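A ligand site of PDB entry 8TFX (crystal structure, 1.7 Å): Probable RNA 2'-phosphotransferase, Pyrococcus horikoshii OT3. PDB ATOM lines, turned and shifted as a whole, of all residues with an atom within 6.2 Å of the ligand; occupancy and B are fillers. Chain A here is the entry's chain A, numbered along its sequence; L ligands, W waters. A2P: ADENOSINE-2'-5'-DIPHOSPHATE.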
ATOM      1  N   ARG A   2       7.834  16.992 -12.397  1.00  0.00           N
ATOM      2  CA  ARG A   2       8.344  16.018 -13.373  1.00  0.00           C
ATOM      3  C   ARG A   2       8.553  14.666 -12.712  1.00  0.00           C
ATOM      4  O   ARG A   2       8.364  13.630 -13.354  1.00  0.00           O
ATOM      5  CB  ARG A   2       9.655  16.520 -13.996  1.00  0.00           C
ATOM      6  CG  ARG A   2       9.421  17.215 -15.383  1.00  0.00           C
ATOM      7  CD  ARG A   2      10.713  17.832 -15.989  1.00  0.00           C
ATOM      8  NE  ARG A   2      11.644  18.237 -14.952  1.00  0.00           N
ATOM      9  CZ  ARG A   2      12.867  17.754 -14.750  1.00  0.00           C
ATOM     10  NH1 ARG A   2      13.310  16.683 -15.397  1.00  0.00           N
ATOM     11  NH2 ARG A   2      13.638  18.305 -13.813  1.00  0.00           N
ATOM     12  N   PHE A   3       8.980  14.673 -11.444  1.00  0.00           N
ATOM     13  CA  PHE A   3       9.197  13.393 -10.759  1.00  0.00           C
ATOM     14  C   PHE A   3       7.894  12.597 -10.642  1.00  0.00           C
ATOM     15  O   PHE A   3       7.847  11.408 -10.988  1.00  0.00           O
ATOM     16  CB  PHE A   3       9.775  13.638  -9.377  1.00  0.00           C
ATOM     17  CG  PHE A   3       9.886  12.367  -8.569  1.00  0.00           C
ATOM     18  CD1 PHE A   3      10.803  11.403  -8.928  1.00  0.00           C
ATOM     19  CD2 PHE A   3       9.016  12.141  -7.503  1.00  0.00           C
ATOM     20  CE1 PHE A   3      10.897  10.200  -8.138  1.00  0.00           C
ATOM     21  CE2 PHE A   3       9.110  10.967  -6.724  1.00  0.00           C
ATOM     22  CZ  PHE A   3      10.043   9.994  -7.068  1.00  0.00           C
ATOM     23  N   SER A   6       6.728  11.538 -14.189  1.00  0.00           N
ATOM     24  CA  SER A   6       7.602  10.487 -14.741  1.00  0.00           C
ATOM     25  C   SER A   6       7.391   9.159 -14.030  1.00  0.00           C
ATOM     26  O   SER A   6       7.393   8.096 -14.674  1.00  0.00           O
ATOM     27  CB  SER A   6       9.077  10.938 -14.633  1.00  0.00           C
ATOM     28  OG  SER A   6       9.970   9.950 -15.189  1.00  0.00           O
ATOM     29  N   LYS A   7       7.224   9.171 -12.699  1.00  0.00           N
ATOM     30  CA  LYS A   7       6.992   7.899 -12.001  1.00  0.00           C
ATOM     31  C   LYS A   7       5.729   7.208 -12.521  1.00  0.00           C
ATOM     32  O   LYS A   7       5.709   5.987 -12.724  1.00  0.00           O
ATOM     33  CB  LYS A   7       6.894   8.132 -10.489  1.00  0.00           C
ATOM     34  CG  LYS A   7       8.205   8.461  -9.828  1.00  0.00           C
ATOM     35  CD  LYS A   7       8.989   7.179  -9.445  1.00  0.00           C
ATOM     36  CE  LYS A   7       8.344   6.517  -8.256  1.00  0.00           C
ATOM     37  NZ  LYS A   7       8.941   5.131  -7.967  1.00  0.00           N
ATOM     38  N   LEU A   8       4.671   7.984 -12.793  1.00  0.00           N
ATOM     39  CA  LEU A   8       3.456   7.385 -13.361  1.00  0.00           C
ATOM     40  C   LEU A   8       3.701   6.887 -14.791  1.00  0.00           C
ATOM     41  O   LEU A   8       3.137   5.865 -15.204  1.00  0.00           O
ATOM     42  CB  LEU A   8       2.316   8.423 -13.322  1.00  0.00           C
ATOM     43  CG  LEU A   8       0.962   7.942 -13.888  1.00  0.00           C
ATOM     44  CD1 LEU A   8       0.413   6.701 -13.140  1.00  0.00           C
ATOM     45  CD2 LEU A   8      -0.106   9.069 -13.872  1.00  0.00           C
ATOM     46  N   MET A   9       4.415   7.685 -15.590  1.00  0.00           N
ATOM     47  CA  MET A   9       4.718   7.283 -16.961  1.00  0.00           C
ATOM     48  C   MET A   9       5.416   5.926 -16.918  1.00  0.00           C
ATOM     49  O   MET A   9       5.125   5.031 -17.729  1.00  0.00           O
ATOM     50  CB  MET A   9       5.672   8.366 -17.457  1.00  0.00           C
ATOM     51  CG  MET A   9       4.869   9.514 -18.164  1.00  0.00           C
ATOM     52  SD  MET A   9       6.095  10.779 -18.606  1.00  0.00           S
ATOM     53  CE  MET A   9       6.957  10.015 -19.969  1.00  0.00           C
ATOM     54  N   ALA A  10       6.401   5.781 -16.021  1.00  0.00           N
ATOM     55  CA  ALA A  10       7.151   4.525 -15.953  1.00  0.00           C
ATOM     56  C   ALA A  10       6.259   3.362 -15.540  1.00  0.00           C
ATOM     57  O   ALA A  10       6.395   2.238 -16.047  1.00  0.00           O
ATOM     58  CB  ALA A  10       8.321   4.655 -14.999  1.00  0.00           C
ATOM     59  N   ARG A  14       5.871   0.518 -18.270  1.00  0.00           N
ATOM     60  CA  ARG A  14       6.583  -0.728 -17.925  1.00  0.00           C
ATOM     61  C   ARG A  14       5.667  -1.816 -17.393  1.00  0.00           C
ATOM     62  O   ARG A  14       5.965  -3.019 -17.559  1.00  0.00           O
ATOM     63  CB  ARG A  14       7.677  -0.476 -16.884  1.00  0.00           C
ATOM     64  CG  ARG A  14       8.814   0.472 -17.329  1.00  0.00           C
ATOM     65  CD  ARG A  14       9.671   0.764 -16.076  1.00  0.00           C
ATOM     66  NE  ARG A  14      10.834   1.587 -16.403  1.00  0.00           N
ATOM     67  CZ  ARG A  14      11.578   2.179 -15.482  1.00  0.00           C
ATOM     68  NH1 ARG A  14      11.295   2.058 -14.188  1.00  0.00           N
ATOM     69  NH2 ARG A  14      12.581   2.984 -15.862  1.00  0.00           N
ATOM     70  N   HIS A  15       4.579  -1.436 -16.714  1.00  0.00           N
ATOM     71  CA  HIS A  15       3.944  -2.439 -15.871  1.00  0.00           C
ATOM     72  C   HIS A  15       2.451  -2.573 -16.088  1.00  0.00           C
ATOM     73  O   HIS A  15       1.937  -3.684 -16.051  1.00  0.00           O
ATOM     74  CB  HIS A  15       4.196  -2.147 -14.391  1.00  0.00           C
ATOM     75  CG  HIS A  15       5.638  -2.125 -14.033  1.00  0.00           C
ATOM     76  ND1 HIS A  15       6.495  -3.185 -14.290  1.00  0.00           N
ATOM     77  CD2 HIS A  15       6.399  -1.139 -13.511  1.00  0.00           C
ATOM     78  CE1 HIS A  15       7.710  -2.865 -13.857  1.00  0.00           C
ATOM     79  NE2 HIS A  15       7.671  -1.632 -13.380  1.00  0.00           N
ATOM     80  N   ASP A  58      15.065  13.473 -19.270  1.00  0.00           N
ATOM     81  CA  ASP A  58      15.264  12.354 -18.326  1.00  0.00           C
ATOM     82  C   ASP A  58      16.739  11.979 -18.193  1.00  0.00           C
ATOM     83  O   ASP A  58      17.448  11.756 -19.178  1.00  0.00           O
ATOM     84  CB  ASP A  58      14.438  11.129 -18.773  1.00  0.00           C
ATOM     85  CG  ASP A  58      14.531   9.999 -17.754  1.00  0.00           C
ATOM     86  OD1 ASP A  58      15.517   9.218 -17.861  1.00  0.00           O
ATOM     87  OD2 ASP A  58      13.651   9.932 -16.850  1.00  0.00           O
ATOM     88  N   GLU A  59      17.207  11.872 -16.931  1.00  0.00           N
ATOM     89  CA  GLU A  59      18.641  11.767 -16.672  1.00  0.00           C
ATOM     90  C   GLU A  59      19.188  10.376 -16.945  1.00  0.00           C
ATOM     91  O   GLU A  59      20.414  10.221 -17.095  1.00  0.00           O
ATOM     92  CB  GLU A  59      18.953  12.182 -15.208  1.00  0.00           C
ATOM     93  CG  GLU A  59      18.292  13.575 -14.712  1.00  0.00           C
ATOM     94  CD  GLU A  59      16.711  13.751 -14.800  1.00  0.00           C
ATOM     95  OE1 GLU A  59      16.238  14.927 -14.858  1.00  0.00           O
ATOM     96  OE2 GLU A  59      15.909  12.761 -14.748  1.00  0.00           O
ATOM     97  N   LYS A  60      18.309   9.384 -17.013  1.00  0.00           N
ATOM     98  CA  LYS A  60      18.703   8.005 -17.275  1.00  0.00           C
ATOM     99  C   LYS A  60      18.423   7.574 -18.699  1.00  0.00           C
ATOM    100  O   LYS A  60      18.847   6.463 -19.070  1.00  0.00           O
ATOM    101  CB  LYS A  60      17.992   7.041 -16.322  1.00  0.00           C
ATOM    102  CG  LYS A  60      18.418   7.201 -14.857  1.00  0.00           C
ATOM    103  CD  LYS A  60      17.969   6.010 -14.006  1.00  0.00           C
ATOM    104  CE  LYS A  60      18.475   6.148 -12.561  1.00  0.00           C
ATOM    105  NZ  LYS A  60      17.972   5.027 -11.686  1.00  0.00           N
ATOM    106  N   ARG A  62      15.289   7.064 -19.699  1.00  0.00           N
ATOM    107  CA  ARG A  62      14.251   6.049 -19.451  1.00  0.00           C
ATOM    108  C   ARG A  62      13.306   5.848 -20.626  1.00  0.00           C
ATOM    109  O   ARG A  62      12.734   4.759 -20.751  1.00  0.00           O
ATOM    110  CB  ARG A  62      13.380   6.405 -18.245  1.00  0.00           C
ATOM    111  CG  ARG A  62      14.143   6.383 -16.931  1.00  0.00           C
ATOM    112  CD  ARG A  62      13.176   6.716 -15.795  1.00  0.00           C
ATOM    113  NE  ARG A  62      13.872   6.638 -14.493  1.00  0.00           N
ATOM    114  CZ  ARG A  62      14.465   7.642 -13.877  1.00  0.00           C
ATOM    115  NH1 ARG A  62      14.415   8.877 -14.365  1.00  0.00           N
ATOM    116  NH2 ARG A  62      15.066   7.430 -12.718  1.00  0.00           N
ATOM    117  N   TYR A  63      13.110   6.873 -21.466  1.00  0.00           N
ATOM    118  CA  TYR A  63      12.030   6.843 -22.435  1.00  0.00           C
ATOM    119  C   TYR A  63      12.552   7.031 -23.856  1.00  0.00           C
ATOM    120  O   TYR A  63      13.659   7.536 -24.087  1.00  0.00           O
ATOM    121  CB  TYR A  63      10.976   7.958 -22.132  1.00  0.00           C
ATOM    122  CG  TYR A  63      10.515   7.893 -20.727  1.00  0.00           C
ATOM    123  CD1 TYR A  63       9.723   6.818 -20.283  1.00  0.00           C
ATOM    124  CD2 TYR A  63      10.869   8.881 -19.811  1.00  0.00           C
ATOM    125  CE1 TYR A  63       9.297   6.748 -18.950  1.00  0.00           C
ATOM    126  CE2 TYR A  63      10.436   8.832 -18.476  1.00  0.00           C
ATOM    127  CZ  TYR A  63       9.651   7.754 -18.074  1.00  0.00           C
ATOM    128  OH  TYR A  63       9.248   7.697 -16.788  1.00  0.00           O
ATOM    129  N   TYR A  74      13.467   0.308 -20.917  1.00  0.00           N
ATOM    130  CA  TYR A  74      13.871  -0.871 -20.147  1.00  0.00           C
ATOM    131  C   TYR A  74      12.918  -0.979 -18.970  1.00  0.00           C
ATOM    132  O   TYR A  74      12.116  -0.070 -18.714  1.00  0.00           O
ATOM    133  CB  TYR A  74      15.330  -0.747 -19.700  1.00  0.00           C
ATOM    134  CG  TYR A  74      15.591   0.463 -18.803  1.00  0.00           C
ATOM    135  CD1 TYR A  74      15.381   0.374 -17.422  1.00  0.00           C
ATOM    136  CD2 TYR A  74      16.086   1.683 -19.329  1.00  0.00           C
ATOM    137  CE1 TYR A  74      15.614   1.472 -16.566  1.00  0.00           C
ATOM    138  CE2 TYR A  74      16.328   2.789 -18.466  1.00  0.00           C
ATOM    139  CZ  TYR A  74      16.056   2.689 -17.104  1.00  0.00           C
ATOM    140  OH  TYR A  74      16.312   3.760 -16.226  1.00  0.00           O
ATOM    141  N   ASN A 129      23.588   1.111  -6.664  1.00  0.00           N
ATOM    142  CA  ASN A 129      22.271   1.622  -6.275  1.00  0.00           C
ATOM    143  C   ASN A 129      21.140   0.702  -6.750  1.00  0.00           C
ATOM    144  O   ASN A 129      20.090   0.616  -6.083  1.00  0.00           O
ATOM    145  CB  ASN A 129      22.103   3.059  -6.774  1.00  0.00           C
ATOM    146  CG  ASN A 129      23.032   4.024  -6.054  1.00  0.00           C
ATOM    147  OD1 ASN A 129      23.429   3.776  -4.920  1.00  0.00           O
ATOM    148  ND2 ASN A 129      23.370   5.142  -6.696  1.00  0.00           N
ATOM    149  N   ARG A 133      18.035  -2.321  -4.303  1.00  0.00           N
ATOM    150  CA  ARG A 133      16.612  -2.595  -4.428  1.00  0.00           C
ATOM    151  C   ARG A 133      16.243  -3.989  -3.912  1.00  0.00           C
ATOM    152  O   ARG A 133      15.071  -4.225  -3.588  1.00  0.00           O
ATOM    153  CB  ARG A 133      16.240  -2.463  -5.913  1.00  0.00           C
ATOM    154  CG  ARG A 133      15.874  -1.086  -6.363  1.00  0.00           C
ATOM    155  CD  ARG A 133      16.082  -0.906  -7.858  1.00  0.00           C
ATOM    156  NE  ARG A 133      16.170   0.502  -8.260  1.00  0.00           N
ATOM    157  CZ  ARG A 133      16.253   0.885  -9.540  1.00  0.00           C
ATOM    158  NH1 ARG A 133      16.192   0.015 -10.515  1.00  0.00           N
ATOM    159  NH2 ARG A 133      16.376   2.176  -9.817  1.00  0.00           N
ATOM    160  N   VAL A 162      22.199   2.164 -18.552  1.00  0.00           N
ATOM    161  CA  VAL A 162      21.722   0.782 -18.478  1.00  0.00           C
ATOM    162  C   VAL A 162      22.069   0.046 -19.774  1.00  0.00           C
ATOM    163  O   VAL A 162      21.908   0.569 -20.871  1.00  0.00           O
ATOM    164  CB  VAL A 162      20.196   0.766 -18.225  1.00  0.00           C
ATOM    165  CG1 VAL A 162      19.624  -0.686 -18.277  1.00  0.00           C
ATOM    166  CG2 VAL A 162      19.873   1.410 -16.922  1.00  0.00           C
HETATM  167  P1  A2P L   1      14.770   3.550 -12.789  1.00  0.00           P
HETATM  168  O1P A2P L   1      15.237   4.633 -11.897  1.00  0.00           O
HETATM  169  O2P A2P L   1      15.676   2.365 -12.625  1.00  0.00           O
HETATM  170  O3P A2P L   1      14.656   3.886 -14.262  1.00  0.00           O
HETATM  171  P2  A2P L   1      14.574   3.510  -6.787  1.00  0.00           P
HETATM  172  O4P A2P L   1      13.850   4.395  -5.814  1.00  0.00           O
HETATM  173  O5P A2P L   1      14.976   2.173  -6.168  1.00  0.00           O
HETATM  174  O6P A2P L   1      15.747   4.230  -7.364  1.00  0.00           O
HETATM  175  O5' A2P L   1      13.457   3.195  -7.954  1.00  0.00           O
HETATM  176  C5' A2P L   1      12.310   2.429  -7.779  1.00  0.00           C
HETATM  177  C4' A2P L   1      11.701   2.331  -9.060  1.00  0.00           C
HETATM  178  O4' A2P L   1      11.088   3.670  -9.363  1.00  0.00           O
HETATM  179  C3' A2P L   1      12.687   2.033 -10.296  1.00  0.00           C
HETATM  180  O3' A2P L   1      11.824   1.212 -11.203  1.00  0.00           O
HETATM  181  C2' A2P L   1      13.035   3.158 -10.822  1.00  0.00           C
HETATM  182  O2' A2P L   1      13.320   3.087 -12.242  1.00  0.00           O
HETATM  183  C1' A2P L   1      11.692   4.085 -10.658  1.00  0.00           C
HETATM  184  N9  A2P L   1      11.901   5.511 -10.782  1.00  0.00           N
HETATM  185  C8  A2P L   1      12.661   6.093  -9.846  1.00  0.00           C
HETATM  186  N7  A2P L   1      12.732   7.430 -10.155  1.00  0.00           N
HETATM  187  C5  A2P L   1      11.997   7.600 -11.312  1.00  0.00           C
HETATM  188  C6  A2P L   1      11.653   8.657 -12.127  1.00  0.00           C
HETATM  189  N6  A2P L   1      12.136   9.981 -11.853  1.00  0.00           N
HETATM  190  N1  A2P L   1      10.876   8.470 -13.183  1.00  0.00           N
HETATM  191  C2  A2P L   1      10.384   7.247 -13.510  1.00  0.00           C
HETATM  192  N3  A2P L   1      10.740   6.207 -12.723  1.00  0.00           N
HETATM  193  C4  A2P L   1      11.497   6.394 -11.647  1.00  0.00           C
HETATM  194  O   HOH W   1      15.814   5.703  -9.286  1.00  0.00           O
HETATM  195  O   HOH W   2      12.154  12.412 -13.414  1.00  0.00           O
HETATM  196  O   HOH W   3       9.176  -0.584 -10.185  1.00  0.00           O
HETATM  197  O   HOH W   4      13.598  -0.159 -12.877  1.00  0.00           O
HETATM  198  O   HOH W   5      14.729   9.168  -8.371  1.00  0.00           O
HETATM  199  O   HOH W   6      17.988   2.202  -4.845  1.00  0.00           O
HETATM  200  O   HOH W   7      11.370   6.057  -6.569  1.00  0.00           O
HETATM  201  O   HOH W   8      13.761   0.654  -4.237  1.00  0.00           O
HETATM  202  O   HOH W   9      13.995   7.202  -6.833  1.00  0.00           O
HETATM  203  O   HOH W  10      14.293  11.110 -10.127  1.00  0.00           O
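OH of Tyr 74 sits at hydrogen-bond distance from O3P of the ligand.
The side-chain hydroxyl (OG) of Ser 6 sits at hydrogen-bond distance from a nitrogen (N1) of the ligand, 2.7 Å away.
The guanidinium group (NH2) of Arg 14 lies within salt-bridge range of an oxygen (O3P) of the ligand.
The side-chain amino group of Lys 60 is in salt-bridge range of an oxygen (O1P) of the ligand, at 2.8 Å.
The guanidinium group of Arg 62 is in salt-bridge range of an oxygen (O3P) of the ligand (2.9 Å).
The guanidinium group of Arg 133 lies within salt-bridge range of an oxygen (O2P) of the ligand (2.9 Å).
The side-chain amino group (NZ) of Lys 7 is in hydrogen-bond range of an oxygen (O4') of the ligand (2.9 Å).
O of Tyr 74 is in hydrogen-bond range of NE of Arg 14 (3.1 Å).
O of Ser 6 is in hydrogen-bond range of OH of Tyr 63 (2.8 Å).
The backbone NH of Lys 60 is in hydrogen-bond range of the side-chain carboxylate of Asp 58, 2.9 Å away.
The guanidinium group of Arg 62 is in salt-bridge range of the side-chain carboxylate of Asp 58 (2.8 Å).
Residues that only touch the ligand: Tyr 63 (3.5 Å), Phe 3 (3.5 Å) and Ala 10 (3.6 Å).
Hydrophobic or aromatic side chains within 4 Å of the ligand: Phe 3, Ala 10 and Tyr 74.
Within 4 Å of the ligand: Phe 3, Ser 6, Lys 7, Ala 10, Arg 14, Lys 60, Arg 62, Tyr 63, Tyr 74 and Arg 133.
Water W1 lies within hydrogen-bond range of an oxygen (O6P) of the ligand (2.4 Å) and the side-chain amino group of Lys 60 (3.3 Å).
Water W4 bridges an oxygen (O3') of the ligand (2.8 Å) and the guanidinium group (NH1) of Arg 14 (3.5 Å).
Water W7 bridges NZ of Lys 7 (3.0 Å) and O4P of the ligand (3.1 Å).
Water W6 bridges O of Asn 129 (2.9 Å) and O5P of the ligand (3.3 Å).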
